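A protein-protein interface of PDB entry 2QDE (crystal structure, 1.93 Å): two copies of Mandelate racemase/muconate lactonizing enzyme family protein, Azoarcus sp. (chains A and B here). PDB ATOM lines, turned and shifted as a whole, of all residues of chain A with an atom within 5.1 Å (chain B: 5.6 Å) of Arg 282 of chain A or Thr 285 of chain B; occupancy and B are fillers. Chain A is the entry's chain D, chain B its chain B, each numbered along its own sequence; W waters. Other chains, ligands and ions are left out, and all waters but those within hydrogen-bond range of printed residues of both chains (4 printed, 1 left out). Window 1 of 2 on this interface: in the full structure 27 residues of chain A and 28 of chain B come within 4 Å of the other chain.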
ATOM      1  N   GLU A  87      20.404  10.710   8.264  1.00  0.00           N
ATOM      2  CA  GLU A  87      19.382  11.581   8.852  1.00  0.00           C
ATOM      3  C   GLU A  87      18.690  12.365   7.733  1.00  0.00           C
ATOM      4  O   GLU A  87      17.465  12.424   7.667  1.00  0.00           O
ATOM      5  CB  GLU A  87      20.004  12.563   9.860  1.00  0.00           C
ATOM      6  CG  GLU A  87      20.286  11.999  11.265  1.00  0.00           C
ATOM      7  CD  GLU A  87      19.081  12.080  12.219  1.00  0.00           C
ATOM      8  OE1 GLU A  87      18.203  12.945  12.018  1.00  0.00           O
ATOM      9  OE2 GLU A  87      19.026  11.290  13.194  1.00  0.00           O
ATOM     10  N   VAL A  90      16.553   9.919   5.244  1.00  0.00           N
ATOM     11  CA  VAL A  90      15.329   9.447   5.878  1.00  0.00           C
ATOM     12  C   VAL A  90      14.326  10.600   5.936  1.00  0.00           C
ATOM     13  O   VAL A  90      13.157  10.427   5.599  1.00  0.00           O
ATOM     14  CB  VAL A  90      15.613   8.894   7.304  1.00  0.00           C
ATOM     15  CG1 VAL A  90      14.316   8.629   8.043  1.00  0.00           C
ATOM     16  CG2 VAL A  90      16.413   7.600   7.196  1.00  0.00           C
ATOM     17  N   ASP A  94      10.533  10.896   4.051  1.00  0.00           N
ATOM     18  CA  ASP A  94       9.297  11.117   4.796  1.00  0.00           C
ATOM     19  C   ASP A  94       8.513  12.321   4.282  1.00  0.00           C
ATOM     20  O   ASP A  94       7.282  12.316   4.292  1.00  0.00           O
ATOM     21  CB  ASP A  94       9.590  11.274   6.296  1.00  0.00           C
ATOM     22  CG  ASP A  94       9.770   9.933   7.002  1.00  0.00           C
ATOM     23  OD1 ASP A  94       9.352   8.900   6.436  1.00  0.00           O
ATOM     24  OD2 ASP A  94      10.313   9.912   8.131  1.00  0.00           O
ATOM     25  N   LEU A 252       5.409   7.320  15.516  1.00  0.00           N
ATOM     26  CA  LEU A 252       5.736   7.965  16.777  1.00  0.00           C
ATOM     27  C   LEU A 252       4.494   8.516  17.448  1.00  0.00           C
ATOM     28  O   LEU A 252       4.349   8.397  18.659  1.00  0.00           O
ATOM     29  CB  LEU A 252       6.730   9.106  16.569  1.00  0.00           C
ATOM     30  CG  LEU A 252       8.136   8.721  16.111  1.00  0.00           C
ATOM     31  CD1 LEU A 252       9.007   9.971  16.103  1.00  0.00           C
ATOM     32  CD2 LEU A 252       8.722   7.677  17.049  1.00  0.00           C
ATOM     33  N   LEU A 278      16.906   3.860  11.624  1.00  0.00           N
ATOM     34  CA  LEU A 278      16.882   5.174  12.250  1.00  0.00           C
ATOM     35  C   LEU A 278      15.492   5.427  12.843  1.00  0.00           C
ATOM     36  O   LEU A 278      15.374   5.778  14.014  1.00  0.00           O
ATOM     37  CB  LEU A 278      17.241   6.276  11.241  1.00  0.00           C
ATOM     38  CG  LEU A 278      17.182   7.710  11.795  1.00  0.00           C
ATOM     39  CD1 LEU A 278      17.925   7.794  13.131  1.00  0.00           C
ATOM     40  CD2 LEU A 278      17.782   8.674  10.790  1.00  0.00           C
ATOM     41  N   LYS A 279      14.446   5.245  12.038  1.00  0.00           N
ATOM     42  CA  LYS A 279      13.078   5.434  12.524  1.00  0.00           C
ATOM     43  C   LYS A 279      12.788   4.488  13.703  1.00  0.00           C
ATOM     44  O   LYS A 279      12.070   4.849  14.632  1.00  0.00           O
ATOM     45  CB  LYS A 279      12.064   5.207  11.389  1.00  0.00           C
ATOM     46  CG  LYS A 279      12.043   6.316  10.327  1.00  0.00           C
ATOM     47  CD  LYS A 279      11.437   7.616  10.869  1.00  0.00           C
ATOM     48  CE  LYS A 279       9.898   7.664  10.712  1.00  0.00           C
ATOM     49  NZ  LYS A 279       9.204   8.040  12.003  1.00  0.00           N
ATOM     50  N   ALA A 280      13.356   3.283  13.668  1.00  0.00           N
ATOM     51  CA  ALA A 280      13.167   2.326  14.758  1.00  0.00           C
ATOM     52  C   ALA A 280      13.825   2.840  16.045  1.00  0.00           C
ATOM     53  O   ALA A 280      13.290   2.651  17.137  1.00  0.00           O
ATOM     54  CB  ALA A 280      13.747   0.960  14.382  1.00  0.00           C
ATOM     55  N   GLN A 281      14.988   3.477  15.918  1.00  0.00           N
ATOM     56  CA  GLN A 281      15.681   4.030  17.084  1.00  0.00           C
ATOM     57  C   GLN A 281      14.769   5.071  17.730  1.00  0.00           C
ATOM     58  O   GLN A 281      14.611   5.112  18.954  1.00  0.00           O
ATOM     59  CB  GLN A 281      17.016   4.678  16.676  1.00  0.00           C
ATOM     60  CG  GLN A 281      18.095   3.678  16.214  1.00  0.00           C
ATOM     61  CD  GLN A 281      19.415   4.353  15.841  1.00  0.00           C
ATOM     62  OE1 GLN A 281      20.405   4.263  16.572  1.00  0.00           O
ATOM     63  NE2 GLN A 281      19.428   5.038  14.707  1.00  0.00           N
ATOM     64  N   ARG A 282      14.164   5.911  16.899  1.00  0.00           N
ATOM     65  CA  ARG A 282      13.245   6.926  17.403  1.00  0.00           C
ATOM     66  C   ARG A 282      12.056   6.226  18.067  1.00  0.00           C
ATOM     67  O   ARG A 282      11.618   6.617  19.149  1.00  0.00           O
ATOM     68  CB  ARG A 282      12.768   7.820  16.254  1.00  0.00           C
ATOM     69  CG  ARG A 282      13.878   8.663  15.628  1.00  0.00           C
ATOM     70  CD  ARG A 282      13.400   9.408  14.389  1.00  0.00           C
ATOM     71  NE  ARG A 282      14.485  10.165  13.769  1.00  0.00           N
ATOM     72  CZ  ARG A 282      14.417  10.741  12.572  1.00  0.00           C
ATOM     73  NH1 ARG A 282      13.310  10.653  11.852  1.00  0.00           N
ATOM     74  NH2 ARG A 282      15.463  11.398  12.089  1.00  0.00           N
ATOM     75  N   TRP A 283      11.550   5.185  17.409  1.00  0.00           N
ATOM     76  CA  TRP A 283      10.417   4.396  17.907  1.00  0.00           C
ATOM     77  C   TRP A 283      10.743   3.909  19.325  1.00  0.00           C
ATOM     78  O   TRP A 283       9.956   4.081  20.261  1.00  0.00           O
ATOM     79  CB  TRP A 283      10.203   3.198  16.975  1.00  0.00           C
ATOM     80  CG  TRP A 283       8.877   2.453  17.086  1.00  0.00           C
ATOM     81  CD1 TRP A 283       7.824   2.525  16.215  1.00  0.00           C
ATOM     82  CD2 TRP A 283       8.526   1.447  18.048  1.00  0.00           C
ATOM     83  NE1 TRP A 283       6.849   1.621  16.565  1.00  0.00           N
ATOM     84  CE2 TRP A 283       7.253   0.946  17.687  1.00  0.00           C
ATOM     85  CE3 TRP A 283       9.168   0.915  19.176  1.00  0.00           C
ATOM     86  CZ2 TRP A 283       6.610  -0.064  18.417  1.00  0.00           C
ATOM     87  CZ3 TRP A 283       8.525  -0.093  19.905  1.00  0.00           C
ATOM     88  CH2 TRP A 283       7.263  -0.569  19.521  1.00  0.00           C
ATOM     89  N   LEU A 284      11.923   3.315  19.471  1.00  0.00           N
ATOM     90  CA  LEU A 284      12.381   2.790  20.753  1.00  0.00           C
ATOM     91  C   LEU A 284      12.608   3.862  21.823  1.00  0.00           C
ATOM     92  O   LEU A 284      12.629   3.554  23.018  1.00  0.00           O
ATOM     93  CB  LEU A 284      13.655   1.958  20.544  1.00  0.00           C
ATOM     94  CG  LEU A 284      13.392   0.635  19.811  1.00  0.00           C
ATOM     95  CD1 LEU A 284      14.705  -0.004  19.378  1.00  0.00           C
ATOM     96  CD2 LEU A 284      12.605  -0.300  20.725  1.00  0.00           C
ATOM     97  N   THR A 285      12.775   5.114  21.401  1.00  0.00           N
ATOM     98  CA  THR A 285      12.964   6.201  22.355  1.00  0.00           C
ATOM     99  C   THR A 285      11.634   6.411  23.059  1.00  0.00           C
ATOM    100  O   THR A 285      11.586   6.610  24.274  1.00  0.00           O
ATOM    101  CB  THR A 285      13.387   7.527  21.664  1.00  0.00           C
ATOM    102  OG1 THR A 285      14.718   7.400  21.150  1.00  0.00           O
ATOM    103  CG2 THR A 285      13.363   8.678  22.652  1.00  0.00           C
ATOM    104  N   LEU A 286      10.551   6.366  22.290  1.00  0.00           N
ATOM    105  CA  LEU A 286       9.227   6.534  22.870  1.00  0.00           C
ATOM    106  C   LEU A 286       8.888   5.341  23.759  1.00  0.00           C
ATOM    107  O   LEU A 286       8.312   5.516  24.834  1.00  0.00           O
ATOM    108  CB  LEU A 286       8.171   6.715  21.774  1.00  0.00           C
ATOM    109  CG  LEU A 286       7.825   8.186  21.495  1.00  0.00           C
ATOM    110  CD1 LEU A 286       9.058   8.931  20.996  1.00  0.00           C
ATOM    111  CD2 LEU A 286       6.720   8.269  20.479  1.00  0.00           C
ATOM    112  N   ALA B 280      20.688  13.631  23.794  1.00  0.00           N
ATOM    113  CA  ALA B 280      20.192  14.761  23.015  1.00  0.00           C
ATOM    114  C   ALA B 280      19.409  14.279  21.793  1.00  0.00           C
ATOM    115  O   ALA B 280      18.411  14.891  21.417  1.00  0.00           O
ATOM    116  CB  ALA B 280      21.350  15.649  22.569  1.00  0.00           C
ATOM    117  N   GLN B 281      19.863  13.195  21.165  1.00  0.00           N
ATOM    118  CA  GLN B 281      19.153  12.665  20.001  1.00  0.00           C
ATOM    119  C   GLN B 281      17.778  12.163  20.448  1.00  0.00           C
ATOM    120  O   GLN B 281      16.783  12.328  19.744  1.00  0.00           O
ATOM    121  CB  GLN B 281      19.939  11.517  19.348  1.00  0.00           C
ATOM    122  CG  GLN B 281      21.262  11.938  18.693  1.00  0.00           C
ATOM    123  CD  GLN B 281      22.019  10.757  18.085  1.00  0.00           C
ATOM    124  OE1 GLN B 281      22.073  10.596  16.858  1.00  0.00           O
ATOM    125  NE2 GLN B 281      22.594   9.922  18.942  1.00  0.00           N
ATOM    126  N   ARG B 282      17.728  11.550  21.624  1.00  0.00           N
ATOM    127  CA  ARG B 282      16.463  11.050  22.153  1.00  0.00           C
ATOM    128  C   ARG B 282      15.554  12.250  22.396  1.00  0.00           C
ATOM    129  O   ARG B 282      14.390  12.253  22.003  1.00  0.00           O
ATOM    130  CB  ARG B 282      16.708  10.273  23.450  1.00  0.00           C
ATOM    131  CG  ARG B 282      17.429   8.950  23.210  1.00  0.00           C
ATOM    132  CD  ARG B 282      17.754   8.217  24.503  1.00  0.00           C
ATOM    133  NE  ARG B 282      18.508   6.994  24.243  1.00  0.00           N
ATOM    134  CZ  ARG B 282      19.104   6.266  25.180  1.00  0.00           C
ATOM    135  NH1 ARG B 282      19.034   6.636  26.452  1.00  0.00           N
ATOM    136  NH2 ARG B 282      19.784   5.174  24.845  1.00  0.00           N
ATOM    137  N   TRP B 283      16.120  13.275  23.020  1.00  0.00           N
ATOM    138  CA  TRP B 283      15.423  14.523  23.324  1.00  0.00           C
ATOM    139  C   TRP B 283      14.822  15.096  22.032  1.00  0.00           C
ATOM    140  O   TRP B 283      13.658  15.513  21.995  1.00  0.00           O
ATOM    141  CB  TRP B 283      16.450  15.503  23.904  1.00  0.00           C
ATOM    142  CG  TRP B 283      15.932  16.689  24.673  1.00  0.00           C
ATOM    143  CD1 TRP B 283      15.969  16.859  26.029  1.00  0.00           C
ATOM    144  CD2 TRP B 283      15.465  17.931  24.127  1.00  0.00           C
ATOM    145  NE1 TRP B 283      15.573  18.136  26.362  1.00  0.00           N
ATOM    146  CE2 TRP B 283      15.256  18.814  25.215  1.00  0.00           C
ATOM    147  CE3 TRP B 283      15.210  18.385  22.826  1.00  0.00           C
ATOM    148  CZ2 TRP B 283      14.802  20.131  25.038  1.00  0.00           C
ATOM    149  CZ3 TRP B 283      14.759  19.693  22.649  1.00  0.00           C
ATOM    150  CH2 TRP B 283      14.561  20.551  23.753  1.00  0.00           C
ATOM    151  N   LEU B 284      15.626  15.099  20.970  1.00  0.00           N
ATOM    152  CA  LEU B 284      15.200  15.630  19.683  1.00  0.00           C
ATOM    153  C   LEU B 284      14.139  14.769  18.994  1.00  0.00           C
ATOM    154  O   LEU B 284      13.438  15.234  18.089  1.00  0.00           O
ATOM    155  CB  LEU B 284      16.424  15.841  18.772  1.00  0.00           C
ATOM    156  CG  LEU B 284      17.346  16.977  19.263  1.00  0.00           C
ATOM    157  CD1 LEU B 284      18.615  17.053  18.424  1.00  0.00           C
ATOM    158  CD2 LEU B 284      16.596  18.303  19.205  1.00  0.00           C
ATOM    159  N   THR B 285      14.017  13.517  19.418  1.00  0.00           N
ATOM    160  CA  THR B 285      13.000  12.647  18.856  1.00  0.00           C
ATOM    161  C   THR B 285      11.657  13.145  19.374  1.00  0.00           C
ATOM    162  O   THR B 285      10.685  13.232  18.630  1.00  0.00           O
ATOM    163  CB  THR B 285      13.198  11.182  19.290  1.00  0.00           C
ATOM    164  OG1 THR B 285      14.380  10.660  18.671  1.00  0.00           O
ATOM    165  CG2 THR B 285      12.000  10.330  18.875  1.00  0.00           C
ATOM    166  N   LEU B 286      11.611  13.470  20.663  1.00  0.00           N
ATOM    167  CA  LEU B 286      10.387  13.972  21.266  1.00  0.00           C
ATOM    168  C   LEU B 286      10.054  15.369  20.743  1.00  0.00           C
ATOM    169  O   LEU B 286       8.883  15.683  20.540  1.00  0.00           O
ATOM    170  CB  LEU B 286      10.498  13.967  22.797  1.00  0.00           C
ATOM    171  CG  LEU B 286      10.114  12.638  23.475  1.00  0.00           C
ATOM    172  CD1 LEU B 286      10.884  11.475  22.870  1.00  0.00           C
ATOM    173  CD2 LEU B 286      10.390  12.719  24.958  1.00  0.00           C
ATOM    174  N   ALA B 287      11.073  16.194  20.499  1.00  0.00           N
ATOM    175  CA  ALA B 287      10.842  17.541  19.969  1.00  0.00           C
ATOM    176  C   ALA B 287      10.193  17.423  18.592  1.00  0.00           C
ATOM    177  O   ALA B 287       9.292  18.189  18.248  1.00  0.00           O
ATOM    178  CB  ALA B 287      12.156  18.308  19.859  1.00  0.00           C
ATOM    179  N   ARG B 288      10.663  16.451  17.816  1.00  0.00           N
ATOM    180  CA  ARG B 288      10.142  16.174  16.483  1.00  0.00           C
ATOM    181  C   ARG B 288       8.664  15.768  16.582  1.00  0.00           C
ATOM    182  O   ARG B 288       7.830  16.220  15.804  1.00  0.00           O
ATOM    183  CB  ARG B 288      10.954  15.040  15.843  1.00  0.00           C
ATOM    184  CG  ARG B 288      10.368  14.474  14.559  1.00  0.00           C
ATOM    185  CD  ARG B 288      11.112  13.207  14.142  1.00  0.00           C
ATOM    186  NE  ARG B 288      12.434  13.487  13.580  1.00  0.00           N
ATOM    187  CZ  ARG B 288      12.630  14.025  12.378  1.00  0.00           C
ATOM    188  NH1 ARG B 288      11.588  14.339  11.621  1.00  0.00           N
ATOM    189  NH2 ARG B 288      13.860  14.245  11.931  1.00  0.00           N
ATOM    190  N   LEU B 289       8.358  14.913  17.550  1.00  0.00           N
ATOM    191  CA  LEU B 289       6.991  14.445  17.776  1.00  0.00           C
ATOM    192  C   LEU B 289       6.075  15.619  18.139  1.00  0.00           C
ATOM    193  O   LEU B 289       4.908  15.655  17.752  1.00  0.00           O
ATOM    194  CB  LEU B 289       6.984  13.402  18.897  1.00  0.00           C
ATOM    195  CG  LEU B 289       5.635  12.891  19.409  1.00  0.00           C
ATOM    196  CD1 LEU B 289       4.826  12.308  18.262  1.00  0.00           C
ATOM    197  CD2 LEU B 289       5.872  11.854  20.487  1.00  0.00           C
ATOM    198  N   ALA B 290       6.619  16.582  18.874  1.00  0.00           N
ATOM    199  CA  ALA B 290       5.857  17.756  19.279  1.00  0.00           C
ATOM    200  C   ALA B 290       5.775  18.771  18.139  1.00  0.00           C
ATOM    201  O   ALA B 290       5.027  19.748  18.219  1.00  0.00           O
ATOM    202  CB  ALA B 290       6.498  18.400  20.512  1.00  0.00           C
ATOM    203  N   ASP B 317      18.568  15.858  11.684  1.00  0.00           N
ATOM    204  CA  ASP B 317      17.593  16.383  10.742  1.00  0.00           C
ATOM    205  C   ASP B 317      16.568  17.336  11.351  1.00  0.00           C
ATOM    206  O   ASP B 317      16.207  18.341  10.742  1.00  0.00           O
ATOM    207  CB  ASP B 317      16.866  15.232  10.049  1.00  0.00           C
ATOM    208  CG  ASP B 317      15.981  15.707   8.921  1.00  0.00           C
ATOM    209  OD1 ASP B 317      16.509  16.310   7.956  1.00  0.00           O
ATOM    210  OD2 ASP B 317      14.763  15.475   8.997  1.00  0.00           O
HETATM  211  O   HOH W   1      21.122   9.547  13.813  1.00  0.00           O
HETATM  212  O   HOH W   2      16.328   8.686  19.129  1.00  0.00           O
HETATM  213  O   HOH W   3      15.395  12.384   9.362  1.00  0.00           O
HETATM  214  O   HOH W   4      21.022  12.713  14.911  1.00  0.00           O
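N of Asp 317 of chain B lies within hydrogen-bond range of OE1 of Glu 87 of chain A (3.0 Å). NH2 of Arg 282 of chain A lies close to NH2 of Arg 288 of chain B (3.3 Å).
The backbone carbonyl oxygen (O) of Gln 281 of chain B sits at hydrogen-bond distance from the side-chain hydroxyl (OG1) of Thr 285 of chain B, 3.1 Å away. The guanidinium group of Arg 288 of chain B lies within salt-bridge range of the side-chain carboxylate of Asp 317 of chain B. The guanidinium group of Arg 282 of chain A is in salt-bridge range of the side-chain carboxylate of Glu 87 of chain A (3.1 Å). The side-chain hydroxyl (OG1) of Thr 285 of chain A lies within hydrogen-bond range of the backbone carbonyl oxygen (O) of Gln 281 of chain A, 3.2 Å away.
Among the printed residues, pairs that only touch across the chains: Leu 286 of chain A with Leu 286 of chain B, Arg 282 of chain A with Thr 285 of chain B, Leu 286 of chain A with Leu 289 of chain B, Thr 285 of chain A with Arg 282 of chain B, Thr 285 of chain A with Leu 286 of chain B, Leu 286 of chain A with Thr 285 of chain B and Leu 252 of chain A with Leu 289 of chain B.
Printed residues of chain B within 4 Å of Leu 252 of chain A: Leu 289. Of the printed residues of chain B, Thr 285 of chain A touches Arg 282 (3.7 Å) and Leu 286 (3.7 Å). Of the printed residues of chain A, Arg 288 of chain B touches Arg 282 (3.3 Å). Of the printed residues of chain A, Leu 289 of chain B touches Leu 252 and Leu 286. The nearest printed residue of chain B that does not touch Leu 252 of chain A is Thr 285 of chain B (4.1 Å).
Hydrophobic or aromatic side chains of chain A that line the printed part of chain B: Leu 286. Of the 12 printed residues of chain B, 6 touch a printed residue of chain A. Printed residues of chain B that touch a printed residue of chain A: Arg 282, Thr 285, Leu 286, Arg 288, Leu 289 and Asp 317. Hydrophobic or aromatic side chains of chain B that line the printed part of chain A: Leu 286 and Leu 289. Among the printed residues, 9 pairs touch across the chains. Among the printed residues, no Asp or Glu carboxylate lies within 4 Å of a Lys or Arg side-chain nitrogen of the other chain.
Arg 282 of chain A touches Thr 285 of chain B, and with the chains exchanged Thr 285 of chain A touches Arg 282 of chain B. Thr 285 of chain A touches Leu 286 of chain B, and with the chains exchanged Leu 286 of chain A touches Thr 285 of chain B. Leu 286 of chain B touches its own counterpart, Leu 286 of chain A. Positions printed for both chains: 280, 281, 282, 283, 284, 285 and 286.
Water W3 lies within hydrogen-bond range of the backbone carbonyl oxygen of Glu 87 of chain A (2.7 Å), the guanidinium group of Arg 282 of chain A (2.9 Å) and the side-chain carboxylate of Asp 317 of chain B (3.2 Å). Water W1 lies within hydrogen-bond range of OE2 of Glu 87 of chain A and OE1 of Gln 281 of chain B. Water W2 lies within hydrogen-bond range of OG1 of Thr 285 of chain B and OG1 of Thr 285 of chain A. Water W4 lies within hydrogen-bond range of the side-chain carboxylate of Glu 87 of chain A and the side-chain amide oxygen of Gln 281 of chain B.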
